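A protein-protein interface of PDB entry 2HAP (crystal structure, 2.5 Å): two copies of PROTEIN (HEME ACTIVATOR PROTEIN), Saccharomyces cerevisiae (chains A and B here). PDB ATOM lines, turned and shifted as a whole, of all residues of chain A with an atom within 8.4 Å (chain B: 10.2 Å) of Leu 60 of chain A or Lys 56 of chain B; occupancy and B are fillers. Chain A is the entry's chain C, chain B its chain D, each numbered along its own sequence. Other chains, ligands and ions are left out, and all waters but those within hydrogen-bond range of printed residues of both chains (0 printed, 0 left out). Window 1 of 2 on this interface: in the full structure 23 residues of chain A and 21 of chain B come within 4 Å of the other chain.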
ATOM      1  N   ALA A  50     -15.829   4.890 -12.231  1.00  0.00           N
ATOM      2  CA  ALA A  50     -16.915   5.823 -11.929  1.00  0.00           C
ATOM      3  C   ALA A  50     -17.032   6.023 -10.425  1.00  0.00           C
ATOM      4  O   ALA A  50     -17.014   7.152  -9.939  1.00  0.00           O
ATOM      5  CB  ALA A  50     -18.223   5.301 -12.484  1.00  0.00           C
ATOM      6  N   LYS A  52     -14.848   5.323  -8.145  1.00  0.00           N
ATOM      7  CA  LYS A  52     -13.589   5.902  -7.719  1.00  0.00           C
ATOM      8  C   LYS A  52     -13.591   7.405  -7.915  1.00  0.00           C
ATOM      9  O   LYS A  52     -13.118   8.147  -7.056  1.00  0.00           O
ATOM     10  CB  LYS A  52     -12.432   5.296  -8.534  1.00  0.00           C
ATOM     11  CG  LYS A  52     -11.215   4.876  -7.722  1.00  0.00           C
ATOM     12  CD  LYS A  52     -11.537   3.701  -6.804  1.00  0.00           C
ATOM     13  CE  LYS A  52     -10.562   2.558  -7.014  1.00  0.00           C
ATOM     14  NZ  LYS A  52      -9.166   3.039  -7.175  1.00  0.00           N
ATOM     15  N   GLU A  53     -14.118   7.850  -9.045  1.00  0.00           N
ATOM     16  CA  GLU A  53     -14.148   9.275  -9.356  1.00  0.00           C
ATOM     17  C   GLU A  53     -15.188  10.024  -8.530  1.00  0.00           C
ATOM     18  O   GLU A  53     -15.022  11.198  -8.219  1.00  0.00           O
ATOM     19  CB  GLU A  53     -14.388   9.475 -10.851  1.00  0.00           C
ATOM     20  CG  GLU A  53     -13.103   9.500 -11.668  1.00  0.00           C
ATOM     21  CD  GLU A  53     -12.163  10.624 -11.243  1.00  0.00           C
ATOM     22  OE1 GLU A  53     -12.664  11.731 -10.909  1.00  0.00           O
ATOM     23  OE2 GLU A  53     -10.927  10.391 -11.244  1.00  0.00           O
ATOM     24  N   LEU A  54     -16.261   9.331  -8.172  1.00  0.00           N
ATOM     25  CA  LEU A  54     -17.318   9.911  -7.361  1.00  0.00           C
ATOM     26  C   LEU A  54     -16.781  10.277  -5.993  1.00  0.00           C
ATOM     27  O   LEU A  54     -17.026  11.365  -5.479  1.00  0.00           O
ATOM     28  CB  LEU A  54     -18.423   8.896  -7.161  1.00  0.00           C
ATOM     29  CG  LEU A  54     -19.847   9.402  -7.076  1.00  0.00           C
ATOM     30  CD1 LEU A  54     -19.955  10.887  -7.494  1.00  0.00           C
ATOM     31  CD2 LEU A  54     -20.679   8.471  -7.960  1.00  0.00           C
ATOM     32  N   LEU A  55     -16.050   9.340  -5.402  1.00  0.00           N
ATOM     33  CA  LEU A  55     -15.464   9.532  -4.082  1.00  0.00           C
ATOM     34  C   LEU A  55     -14.382  10.590  -4.136  1.00  0.00           C
ATOM     35  O   LEU A  55     -14.162  11.303  -3.172  1.00  0.00           O
ATOM     36  CB  LEU A  55     -14.860   8.230  -3.582  1.00  0.00           C
ATOM     37  CG  LEU A  55     -15.816   7.040  -3.375  1.00  0.00           C
ATOM     38  CD1 LEU A  55     -14.979   5.773  -3.366  1.00  0.00           C
ATOM     39  CD2 LEU A  55     -16.621   7.133  -2.062  1.00  0.00           C
ATOM     40  N   LYS A  56     -13.672  10.668  -5.254  1.00  0.00           N
ATOM     41  CA  LYS A  56     -12.632  11.671  -5.394  1.00  0.00           C
ATOM     42  C   LYS A  56     -13.351  13.004  -5.358  1.00  0.00           C
ATOM     43  O   LYS A  56     -12.913  13.949  -4.703  1.00  0.00           O
ATOM     44  CB  LYS A  56     -11.918  11.510  -6.737  1.00  0.00           C
ATOM     45  CG  LYS A  56     -10.435  11.311  -6.607  1.00  0.00           C
ATOM     46  CD  LYS A  56      -9.860  10.672  -7.857  1.00  0.00           C
ATOM     47  CE  LYS A  56      -9.319  11.728  -8.809  1.00  0.00           C
ATOM     48  NZ  LYS A  56      -9.357  13.071  -8.164  1.00  0.00           N
ATOM     49  N   ASP A  57     -14.484  13.056  -6.049  1.00  0.00           N
ATOM     50  CA  ASP A  57     -15.299  14.253  -6.124  1.00  0.00           C
ATOM     51  C   ASP A  57     -15.662  14.796  -4.751  1.00  0.00           C
ATOM     52  O   ASP A  57     -15.431  15.972  -4.453  1.00  0.00           O
ATOM     53  CB  ASP A  57     -16.581  13.960  -6.897  1.00  0.00           C
ATOM     54  CG  ASP A  57     -16.392  14.101  -8.384  1.00  0.00           C
ATOM     55  OD1 ASP A  57     -15.301  14.552  -8.769  1.00  0.00           O
ATOM     56  OD2 ASP A  57     -17.305  13.769  -9.170  1.00  0.00           O
ATOM     57  N   ASN A  58     -16.218  13.922  -3.915  1.00  0.00           N
ATOM     58  CA  ASN A  58     -16.648  14.301  -2.573  1.00  0.00           C
ATOM     59  C   ASN A  58     -15.519  14.867  -1.734  1.00  0.00           C
ATOM     60  O   ASN A  58     -15.717  15.831  -0.988  1.00  0.00           O
ATOM     61  CB  ASN A  58     -17.259  13.109  -1.838  1.00  0.00           C
ATOM     62  CG  ASN A  58     -18.174  13.530  -0.701  1.00  0.00           C
ATOM     63  OD1 ASN A  58     -18.453  14.713  -0.507  1.00  0.00           O
ATOM     64  ND2 ASN A  58     -18.653  12.554   0.055  1.00  0.00           N
ATOM     65  N   GLU A  59     -14.342  14.261  -1.847  1.00  0.00           N
ATOM     66  CA  GLU A  59     -13.178  14.700  -1.093  1.00  0.00           C
ATOM     67  C   GLU A  59     -12.816  16.110  -1.538  1.00  0.00           C
ATOM     68  O   GLU A  59     -12.396  16.948  -0.731  1.00  0.00           O
ATOM     69  CB  GLU A  59     -11.986  13.755  -1.341  1.00  0.00           C
ATOM     70  CG  GLU A  59     -11.213  13.360  -0.086  1.00  0.00           C
ATOM     71  CD  GLU A  59      -9.742  13.075  -0.364  1.00  0.00           C
ATOM     72  OE1 GLU A  59      -9.380  12.911  -1.546  1.00  0.00           O
ATOM     73  OE2 GLU A  59      -8.949  13.013   0.610  1.00  0.00           O
ATOM     74  N   LEU A  60     -12.994  16.371  -2.829  1.00  0.00           N
ATOM     75  CA  LEU A  60     -12.695  17.677  -3.396  1.00  0.00           C
ATOM     76  C   LEU A  60     -13.601  18.752  -2.777  1.00  0.00           C
ATOM     77  O   LEU A  60     -13.129  19.799  -2.341  1.00  0.00           O
ATOM     78  CB  LEU A  60     -12.891  17.645  -4.914  1.00  0.00           C
ATOM     79  CG  LEU A  60     -12.237  18.758  -5.736  1.00  0.00           C
ATOM     80  CD1 LEU A  60     -10.932  19.153  -5.072  1.00  0.00           C
ATOM     81  CD2 LEU A  60     -11.989  18.283  -7.161  1.00  0.00           C
ATOM     82  N   LYS A  61     -14.900  18.468  -2.735  1.00  0.00           N
ATOM     83  CA  LYS A  61     -15.896  19.387  -2.188  1.00  0.00           C
ATOM     84  C   LYS A  61     -15.650  19.676  -0.714  1.00  0.00           C
ATOM     85  O   LYS A  61     -15.700  20.827  -0.291  1.00  0.00           O
ATOM     86  CB  LYS A  61     -17.310  18.817  -2.371  1.00  0.00           C
ATOM     87  CG  LYS A  61     -18.113  19.429  -3.535  1.00  0.00           C
ATOM     88  CD  LYS A  61     -18.719  20.803  -3.179  1.00  0.00           C
ATOM     89  CE  LYS A  61     -20.216  20.719  -2.818  1.00  0.00           C
ATOM     90  NZ  LYS A  61     -20.661  21.840  -1.927  1.00  0.00           N
ATOM     91  N   LYS A  62     -15.364  18.638   0.065  1.00  0.00           N
ATOM     92  CA  LYS A  62     -15.128  18.836   1.484  1.00  0.00           C
ATOM     93  C   LYS A  62     -13.808  19.546   1.732  1.00  0.00           C
ATOM     94  O   LYS A  62     -13.729  20.425   2.587  1.00  0.00           O
ATOM     95  CB  LYS A  62     -15.122  17.501   2.222  1.00  0.00           C
ATOM     96  CG  LYS A  62     -16.419  16.752   2.140  1.00  0.00           C
ATOM     97  CD  LYS A  62     -16.154  15.266   2.035  1.00  0.00           C
ATOM     98  CE  LYS A  62     -16.744  14.493   3.193  1.00  0.00           C
ATOM     99  NZ  LYS A  62     -16.486  13.060   2.927  1.00  0.00           N
ATOM    100  N   LEU A  63     -12.771  19.163   0.989  1.00  0.00           N
ATOM    101  CA  LEU A  63     -11.447  19.769   1.144  1.00  0.00           C
ATOM    102  C   LEU A  63     -11.472  21.244   0.787  1.00  0.00           C
ATOM    103  O   LEU A  63     -10.847  22.061   1.464  1.00  0.00           O
ATOM    104  CB  LEU A  63     -10.417  19.043   0.278  1.00  0.00           C
ATOM    105  CG  LEU A  63      -9.074  18.660   0.918  1.00  0.00           C
ATOM    106  CD1 LEU A  63      -7.999  18.705  -0.146  1.00  0.00           C
ATOM    107  CD2 LEU A  63      -8.731  19.584   2.070  1.00  0.00           C
ATOM    108  N   ARG A  64     -12.190  21.585  -0.280  1.00  0.00           N
ATOM    109  CA  ARG A  64     -12.310  22.980  -0.688  1.00  0.00           C
ATOM    110  C   ARG A  64     -13.053  23.765   0.402  1.00  0.00           C
ATOM    111  O   ARG A  64     -12.643  24.866   0.764  1.00  0.00           O
ATOM    112  CB  ARG A  64     -13.083  23.104  -2.004  1.00  0.00           C
ATOM    113  CG  ARG A  64     -12.702  24.341  -2.824  1.00  0.00           C
ATOM    114  CD  ARG A  64     -13.167  24.245  -4.281  1.00  0.00           C
ATOM    115  NE  ARG A  64     -14.305  23.337  -4.404  1.00  0.00           N
ATOM    116  CZ  ARG A  64     -14.433  22.399  -5.332  1.00  0.00           C
ATOM    117  NH1 ARG A  64     -13.488  22.224  -6.245  1.00  0.00           N
ATOM    118  NH2 ARG A  64     -15.500  21.614  -5.330  1.00  0.00           N
ATOM    119  N   GLU A  65     -14.137  23.191   0.923  1.00  0.00           N
ATOM    120  CA  GLU A  65     -14.947  23.836   1.959  1.00  0.00           C
ATOM    121  C   GLU A  65     -14.177  23.955   3.279  1.00  0.00           C
ATOM    122  O   GLU A  65     -14.373  24.897   4.045  1.00  0.00           O
ATOM    123  CB  GLU A  65     -16.242  23.043   2.160  1.00  0.00           C
ATOM    124  CG  GLU A  65     -17.437  23.629   1.394  1.00  0.00           C
ATOM    125  CD  GLU A  65     -18.571  22.626   1.148  1.00  0.00           C
ATOM    126  OE1 GLU A  65     -18.875  21.810   2.050  1.00  0.00           O
ATOM    127  OE2 GLU A  65     -19.160  22.662   0.038  1.00  0.00           O
ATOM    128  N   ARG A  66     -13.291  22.995   3.522  1.00  0.00           N
ATOM    129  CA  ARG A  66     -12.468  22.973   4.721  1.00  0.00           C
ATOM    130  C   ARG A  66     -11.383  24.021   4.547  1.00  0.00           C
ATOM    131  O   ARG A  66     -11.014  24.714   5.494  1.00  0.00           O
ATOM    132  CB  ARG A  66     -11.822  21.595   4.897  1.00  0.00           C
ATOM    133  CG  ARG A  66     -10.778  21.512   6.014  1.00  0.00           C
ATOM    134  CD  ARG A  66     -11.364  21.974   7.325  1.00  0.00           C
ATOM    135  NE  ARG A  66     -10.502  21.683   8.469  1.00  0.00           N
ATOM    136  CZ  ARG A  66     -10.824  21.985   9.724  1.00  0.00           C
ATOM    137  NH1 ARG A  66     -11.972  22.591   9.985  1.00  0.00           N
ATOM    138  NH2 ARG A  66     -10.014  21.667  10.714  1.00  0.00           N
ATOM    139  N   VAL A  67     -10.882  24.145   3.328  1.00  0.00           N
ATOM    140  CA  VAL A  67      -9.845  25.125   3.075  1.00  0.00           C
ATOM    141  C   VAL A  67     -10.424  26.526   3.199  1.00  0.00           C
ATOM    142  O   VAL A  67      -9.805  27.408   3.786  1.00  0.00           O
ATOM    143  CB  VAL A  67      -9.231  24.964   1.676  1.00  0.00           C
ATOM    144  CG1 VAL A  67      -8.482  26.224   1.297  1.00  0.00           C
ATOM    145  CG2 VAL A  67      -8.277  23.793   1.665  1.00  0.00           C
ATOM    146  N   GLU B  48     -13.146  16.027 -22.937  1.00  0.00           N
ATOM    147  CA  GLU B  48     -13.997  16.526 -21.857  1.00  0.00           C
ATOM    148  C   GLU B  48     -13.659  15.933 -20.501  1.00  0.00           C
ATOM    149  O   GLU B  48     -13.179  16.631 -19.600  1.00  0.00           O
ATOM    150  CB  GLU B  48     -15.459  16.217 -22.174  1.00  0.00           C
ATOM    151  CG  GLU B  48     -16.389  17.391 -21.960  1.00  0.00           C
ATOM    152  CD  GLU B  48     -15.961  18.619 -22.754  1.00  0.00           C
ATOM    153  OE1 GLU B  48     -14.787  19.048 -22.626  1.00  0.00           O
ATOM    154  OE2 GLU B  48     -16.805  19.157 -23.506  1.00  0.00           O
ATOM    155  N   GLU B  49     -13.956  14.646 -20.354  1.00  0.00           N
ATOM    156  CA  GLU B  49     -13.692  13.930 -19.115  1.00  0.00           C
ATOM    157  C   GLU B  49     -12.242  14.142 -18.786  1.00  0.00           C
ATOM    158  O   GLU B  49     -11.892  14.552 -17.688  1.00  0.00           O
ATOM    159  CB  GLU B  49     -13.950  12.426 -19.268  1.00  0.00           C
ATOM    160  CG  GLU B  49     -15.300  12.064 -19.863  1.00  0.00           C
ATOM    161  CD  GLU B  49     -15.265  11.891 -21.386  1.00  0.00           C
ATOM    162  OE1 GLU B  49     -14.799  12.805 -22.113  1.00  0.00           O
ATOM    163  OE2 GLU B  49     -15.720  10.826 -21.857  1.00  0.00           O
ATOM    164  N   ALA B  50     -11.400  13.870 -19.767  1.00  0.00           N
ATOM    165  CA  ALA B  50      -9.968  14.017 -19.616  1.00  0.00           C
ATOM    166  C   ALA B  50      -9.605  15.350 -18.955  1.00  0.00           C
ATOM    167  O   ALA B  50      -8.918  15.394 -17.931  1.00  0.00           O
ATOM    168  CB  ALA B  50      -9.321  13.911 -20.968  1.00  0.00           C
ATOM    169  N   GLU B  51     -10.062  16.440 -19.557  1.00  0.00           N
ATOM    170  CA  GLU B  51      -9.759  17.769 -19.045  1.00  0.00           C
ATOM    171  C   GLU B  51     -10.351  18.079 -17.684  1.00  0.00           C
ATOM    172  O   GLU B  51      -9.712  18.759 -16.885  1.00  0.00           O
ATOM    173  CB  GLU B  51     -10.196  18.830 -20.050  1.00  0.00           C
ATOM    174  CG  GLU B  51      -9.198  19.979 -20.198  1.00  0.00           C
ATOM    175  CD  GLU B  51      -8.165  19.746 -21.297  1.00  0.00           C
ATOM    176  OE1 GLU B  51      -8.561  19.632 -22.482  1.00  0.00           O
ATOM    177  OE2 GLU B  51      -6.955  19.690 -20.968  1.00  0.00           O
ATOM    178  N   LYS B  52     -11.561  17.583 -17.414  1.00  0.00           N
ATOM    179  CA  LYS B  52     -12.214  17.838 -16.129  1.00  0.00           C
ATOM    180  C   LYS B  52     -11.495  17.123 -14.988  1.00  0.00           C
ATOM    181  O   LYS B  52     -11.419  17.633 -13.873  1.00  0.00           O
ATOM    182  CB  LYS B  52     -13.679  17.397 -16.162  1.00  0.00           C
ATOM    183  CG  LYS B  52     -14.464  17.716 -14.881  1.00  0.00           C
ATOM    184  CD  LYS B  52     -14.681  19.233 -14.685  1.00  0.00           C
ATOM    185  CE  LYS B  52     -14.263  19.685 -13.266  1.00  0.00           C
ATOM    186  NZ  LYS B  52     -13.881  21.138 -13.133  1.00  0.00           N
ATOM    187  N   GLU B  53     -10.980  15.930 -15.265  1.00  0.00           N
ATOM    188  CA  GLU B  53     -10.238  15.167 -14.268  1.00  0.00           C
ATOM    189  C   GLU B  53      -8.823  15.712 -14.102  1.00  0.00           C
ATOM    190  O   GLU B  53      -8.173  15.534 -13.068  1.00  0.00           O
ATOM    191  CB  GLU B  53     -10.180  13.708 -14.674  1.00  0.00           C
ATOM    192  CG  GLU B  53     -11.171  12.873 -13.917  1.00  0.00           C
ATOM    193  CD  GLU B  53     -11.859  11.871 -14.804  1.00  0.00           C
ATOM    194  OE1 GLU B  53     -11.205  10.878 -15.178  1.00  0.00           O
ATOM    195  OE2 GLU B  53     -13.054  12.073 -15.131  1.00  0.00           O
ATOM    196  N   LEU B  54      -8.328  16.354 -15.142  1.00  0.00           N
ATOM    197  CA  LEU B  54      -7.017  16.959 -15.074  1.00  0.00           C
ATOM    198  C   LEU B  54      -7.133  18.115 -14.078  1.00  0.00           C
ATOM    199  O   LEU B  54      -6.211  18.386 -13.312  1.00  0.00           O
ATOM    200  CB  LEU B  54      -6.615  17.457 -16.461  1.00  0.00           C
ATOM    201  CG  LEU B  54      -5.414  18.392 -16.537  1.00  0.00           C
ATOM    202  CD1 LEU B  54      -4.242  17.807 -15.788  1.00  0.00           C
ATOM    203  CD2 LEU B  54      -5.061  18.620 -18.009  1.00  0.00           C
ATOM    204  N   LEU B  55      -8.281  18.787 -14.077  1.00  0.00           N
ATOM    205  CA  LEU B  55      -8.504  19.902 -13.142  1.00  0.00           C
ATOM    206  C   LEU B  55      -8.769  19.402 -11.712  1.00  0.00           C
ATOM    207  O   LEU B  55      -8.189  19.912 -10.750  1.00  0.00           O
ATOM    208  CB  LEU B  55      -9.690  20.733 -13.598  1.00  0.00           C
ATOM    209  CG  LEU B  55      -9.430  21.868 -14.574  1.00  0.00           C
ATOM    210  CD1 LEU B  55      -8.273  21.532 -15.486  1.00  0.00           C
ATOM    211  CD2 LEU B  55     -10.682  22.080 -15.376  1.00  0.00           C
ATOM    212  N   LYS B  56      -9.658  18.416 -11.588  1.00  0.00           N
ATOM    213  CA  LYS B  56      -9.983  17.828 -10.295  1.00  0.00           C
ATOM    214  C   LYS B  56      -8.672  17.423  -9.640  1.00  0.00           C
ATOM    215  O   LYS B  56      -8.378  17.807  -8.520  1.00  0.00           O
ATOM    216  CB  LYS B  56     -10.834  16.575 -10.473  1.00  0.00           C
ATOM    217  CG  LYS B  56     -12.315  16.800 -10.688  1.00  0.00           C
ATOM    218  CD  LYS B  56     -13.104  15.650 -10.087  1.00  0.00           C
ATOM    219  CE  LYS B  56     -13.468  14.596 -11.127  1.00  0.00           C
ATOM    220  NZ  LYS B  56     -14.754  14.929 -11.815  1.00  0.00           N
ATOM    221  N   ASP B  57      -7.891  16.640 -10.370  1.00  0.00           N
ATOM    222  CA  ASP B  57      -6.605  16.151  -9.887  1.00  0.00           C
ATOM    223  C   ASP B  57      -5.723  17.253  -9.322  1.00  0.00           C
ATOM    224  O   ASP B  57      -5.293  17.206  -8.169  1.00  0.00           O
ATOM    225  CB  ASP B  57      -5.857  15.459 -11.025  1.00  0.00           C
ATOM    226  CG  ASP B  57      -6.148  13.971 -11.100  1.00  0.00           C
ATOM    227  OD1 ASP B  57      -6.884  13.446 -10.237  1.00  0.00           O
ATOM    228  OD2 ASP B  57      -5.638  13.313 -12.029  1.00  0.00           O
ATOM    229  N   ASN B  58      -5.434  18.233 -10.163  1.00  0.00           N
ATOM    230  CA  ASN B  58      -4.582  19.348  -9.776  1.00  0.00           C
ATOM    231  C   ASN B  58      -5.067  20.136  -8.578  1.00  0.00           C
ATOM    232  O   ASN B  58      -4.261  20.671  -7.836  1.00  0.00           O
ATOM    233  CB  ASN B  58      -4.399  20.286 -10.962  1.00  0.00           C
ATOM    234  CG  ASN B  58      -3.364  19.780 -11.939  1.00  0.00           C
ATOM    235  OD1 ASN B  58      -2.176  20.054 -11.800  1.00  0.00           O
ATOM    236  ND2 ASN B  58      -3.809  19.034 -12.932  1.00  0.00           N
ATOM    237  N   GLU B  59      -6.383  20.203  -8.396  1.00  0.00           N
ATOM    238  CA  GLU B  59      -6.960  20.940  -7.279  1.00  0.00           C
ATOM    239  C   GLU B  59      -6.865  20.172  -5.982  1.00  0.00           C
ATOM    240  O   GLU B  59      -6.494  20.751  -4.968  1.00  0.00           O
ATOM    241  CB  GLU B  59      -8.412  21.279  -7.550  1.00  0.00           C
ATOM    242  CG  GLU B  59      -8.923  22.440  -6.727  1.00  0.00           C
ATOM    243  CD  GLU B  59     -10.416  22.609  -6.849  1.00  0.00           C
ATOM    244  OE1 GLU B  59     -10.984  22.066  -7.816  1.00  0.00           O
ATOM    245  OE2 GLU B  59     -11.029  23.279  -5.989  1.00  0.00           O
ATOM    246  N   LEU B  60      -7.185  18.880  -5.994  1.00  0.00           N
ATOM    247  CA  LEU B  60      -7.116  18.115  -4.747  1.00  0.00           C
ATOM    248  C   LEU B  60      -5.688  18.162  -4.239  1.00  0.00           C
ATOM    249  O   LEU B  60      -5.438  18.245  -3.043  1.00  0.00           O
ATOM    250  CB  LEU B  60      -7.540  16.625  -4.916  1.00  0.00           C
ATOM    251  CG  LEU B  60      -8.350  16.157  -3.711  1.00  0.00           C
ATOM    252  N   LYS B  61      -4.749  18.139  -5.166  1.00  0.00           N
ATOM    253  CA  LYS B  61      -3.344  18.180  -4.835  1.00  0.00           C
ATOM    254  C   LYS B  61      -2.989  19.501  -4.165  1.00  0.00           C
ATOM    255  O   LYS B  61      -2.439  19.524  -3.067  1.00  0.00           O
ATOM    256  CB  LYS B  61      -2.548  17.998  -6.116  1.00  0.00           C
ATOM    257  CG  LYS B  61      -1.078  17.953  -5.921  1.00  0.00           C
ATOM    258  CD  LYS B  61      -0.408  17.919  -7.266  1.00  0.00           C
ATOM    259  CE  LYS B  61       1.058  18.237  -7.132  1.00  0.00           C
ATOM    260  NZ  LYS B  61       1.393  18.307  -5.686  1.00  0.00           N
ATOM    261  N   LYS B  62      -3.313  20.609  -4.822  1.00  0.00           N
ATOM    262  CA  LYS B  62      -3.030  21.937  -4.281  1.00  0.00           C
ATOM    263  C   LYS B  62      -3.809  22.181  -2.985  1.00  0.00           C
ATOM    264  O   LYS B  62      -3.254  22.672  -2.002  1.00  0.00           O
ATOM    265  CB  LYS B  62      -3.383  23.010  -5.313  1.00  0.00           C
ATOM    266  CG  LYS B  62      -2.291  23.293  -6.333  1.00  0.00           C
ATOM    267  CD  LYS B  62      -0.968  23.661  -5.659  1.00  0.00           C
ATOM    268  CE  LYS B  62      -0.396  24.985  -6.181  1.00  0.00           C
ATOM    269  NZ  LYS B  62      -0.118  25.990  -5.102  1.00  0.00           N
ATOM    270  N   LEU B  63      -5.095  21.829  -2.984  1.00  0.00           N
ATOM    271  CA  LEU B  63      -5.942  22.032  -1.810  1.00  0.00           C
ATOM    272  C   LEU B  63      -5.396  21.282  -0.617  1.00  0.00           C
ATOM    273  O   LEU B  63      -5.566  21.707   0.520  1.00  0.00           O
ATOM    274  CB  LEU B  63      -7.368  21.544  -2.054  1.00  0.00           C
ATOM    275  CG  LEU B  63      -8.337  22.473  -2.786  1.00  0.00           C
ATOM    276  CD1 LEU B  63      -9.719  21.903  -2.664  1.00  0.00           C
ATOM    277  CD2 LEU B  63      -8.291  23.884  -2.236  1.00  0.00           C
ATOM    278  N   ARG B  64      -4.732  20.164  -0.882  1.00  0.00           N
ATOM    279  CA  ARG B  64      -4.183  19.336   0.181  1.00  0.00           C
ATOM    280  C   ARG B  64      -2.955  19.945   0.818  1.00  0.00           C
ATOM    281  O   ARG B  64      -2.827  19.957   2.040  1.00  0.00           O
ATOM    282  CB  ARG B  64      -3.831  17.948  -0.353  1.00  0.00           C
ATOM    283  CG  ARG B  64      -4.983  16.994  -0.353  1.00  0.00           C
ATOM    284  CD  ARG B  64      -4.484  15.582  -0.247  1.00  0.00           C
ATOM    285  NE  ARG B  64      -5.076  14.733  -1.267  1.00  0.00           N
ATOM    286  CZ  ARG B  64      -6.252  14.131  -1.136  1.00  0.00           C
ATOM    287  NH1 ARG B  64      -6.954  14.275  -0.014  1.00  0.00           N
ATOM    288  NH2 ARG B  64      -6.732  13.403  -2.132  1.00  0.00           N
ATOM    289  N   VAL B  67      -4.210  23.153   2.887  1.00  0.00           N
ATOM    290  CA  VAL B  67      -4.816  22.920   4.193  1.00  0.00           C
ATOM    291  C   VAL B  67      -3.704  22.749   5.227  1.00  0.00           C
ATOM    292  O   VAL B  67      -3.844  23.164   6.370  1.00  0.00           O
ATOM    293  CB  VAL B  67      -5.733  21.659   4.195  1.00  0.00           C
ATOM    294  CG1 VAL B  67      -5.357  20.736   5.306  1.00  0.00           C
ATOM    295  CG2 VAL B  67      -7.173  22.068   4.382  1.00  0.00           C
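Hydrophobic or aromatic side chains of chain B within 4 Å of the printed part of chain A: Leu 63 and Val 67.
Hydrophobic or aromatic side chains of chain A within 4 Å of the printed part of chain B: Leu 60, Leu 63 and Val 67.
Among the printed residues, Asp or Glu carboxylates within 4 Å of a Lys or Arg side-chain nitrogen of the other chain: Glu 53 of chain A with Lys 56 of chain B, Lys 56 of chain A with Asp 57 of chain B, Asp 57 of chain A with Lys 56 of chain B, Glu 59 of chain A with Arg 64 of chain B and Arg 64 of chain A with Glu 59 of chain B.
The side-chain carboxylate (OE1) of Glu 53 of chain A is in salt-bridge range of the side-chain amino group (NZ) of Lys 56 of chain B (3.9 Å).
The side-chain amino group (NZ) of Lys 56 of chain A is in salt-bridge range of the side-chain carboxylate (OD1) of Asp 57 of chain B, at 3.2 Å.
OD1 of Asp 57 of chain A lies within salt-bridge range of NZ of Lys 56 of chain B (3.1 Å).
The guanidinium group (NH1) of Arg 64 of chain B lies within salt-bridge range of the side-chain carboxylate (OE2) of Glu 59 of chain A (2.4 Å).
The guanidinium group of Arg 64 of chain A lies within salt-bridge range of the side-chain carboxylate of Glu 59 of chain B (2.7 Å).
Printed residues of chain B within 4 Å of Lys 56 of chain A: Asp 57 (3.2 Å).
Asp 57 of chain A touches just one residue of chain B: Lys 56 (2.8 Å).
Arg 64 of chain A touches two residues of chain B.
Of chain A, only Glu 53, Asp 57 and Leu 60 come within 4 Å of Lys 56 of chain B.
Printed residues of chain A within 4 Å of Asp 57 of chain B: Lys 56 (3.2 Å).
Of the printed residues of chain A, Leu 60 of chain B touches Leu 60 and Leu 63.
Among the printed residues, pairs that only touch across the chains: Val 67 of chain A with Val 67 of chain B, Arg 64 of chain A with Leu 63 of chain B, Leu 63 of chain A with Arg 64 of chain B, Leu 63 of chain A with Leu 63 of chain B, Glu 53 of chain A with Glu 53 of chain B, Val 67 of chain A with Leu 63 of chain B, Leu 63 of chain A with Val 67 of chain B, Leu 60 of chain A with Lys 56 of chain B, Leu 60 of chain A with Leu 63 of chain B, Leu 60 of chain A with Leu 60 of chain B, Leu 63 of chain A with Leu 60 of chain B, Leu 60 of chain A with Glu 59 of chain B and Arg 66 of chain A with Val 67 of chain B.
Glu 53 of chain A touches Lys 56 of chain B, but with the chains exchanged Lys 56 of chain A does not touch Glu 53 of chain B (5.6 Å).
Leu 60 of chain A touches Glu 59 of chain B, but with the chains exchanged Glu 59 of chain A does not touch Leu 60 of chain B (4.04 Å).
Leu 60 of chain A touches its own counterpart, Leu 60 of chain B.
Leu 60 of chain A touches Leu 63 of chain B, and with the chains exchanged Leu 63 of chain A touches Leu 60 of chain B.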
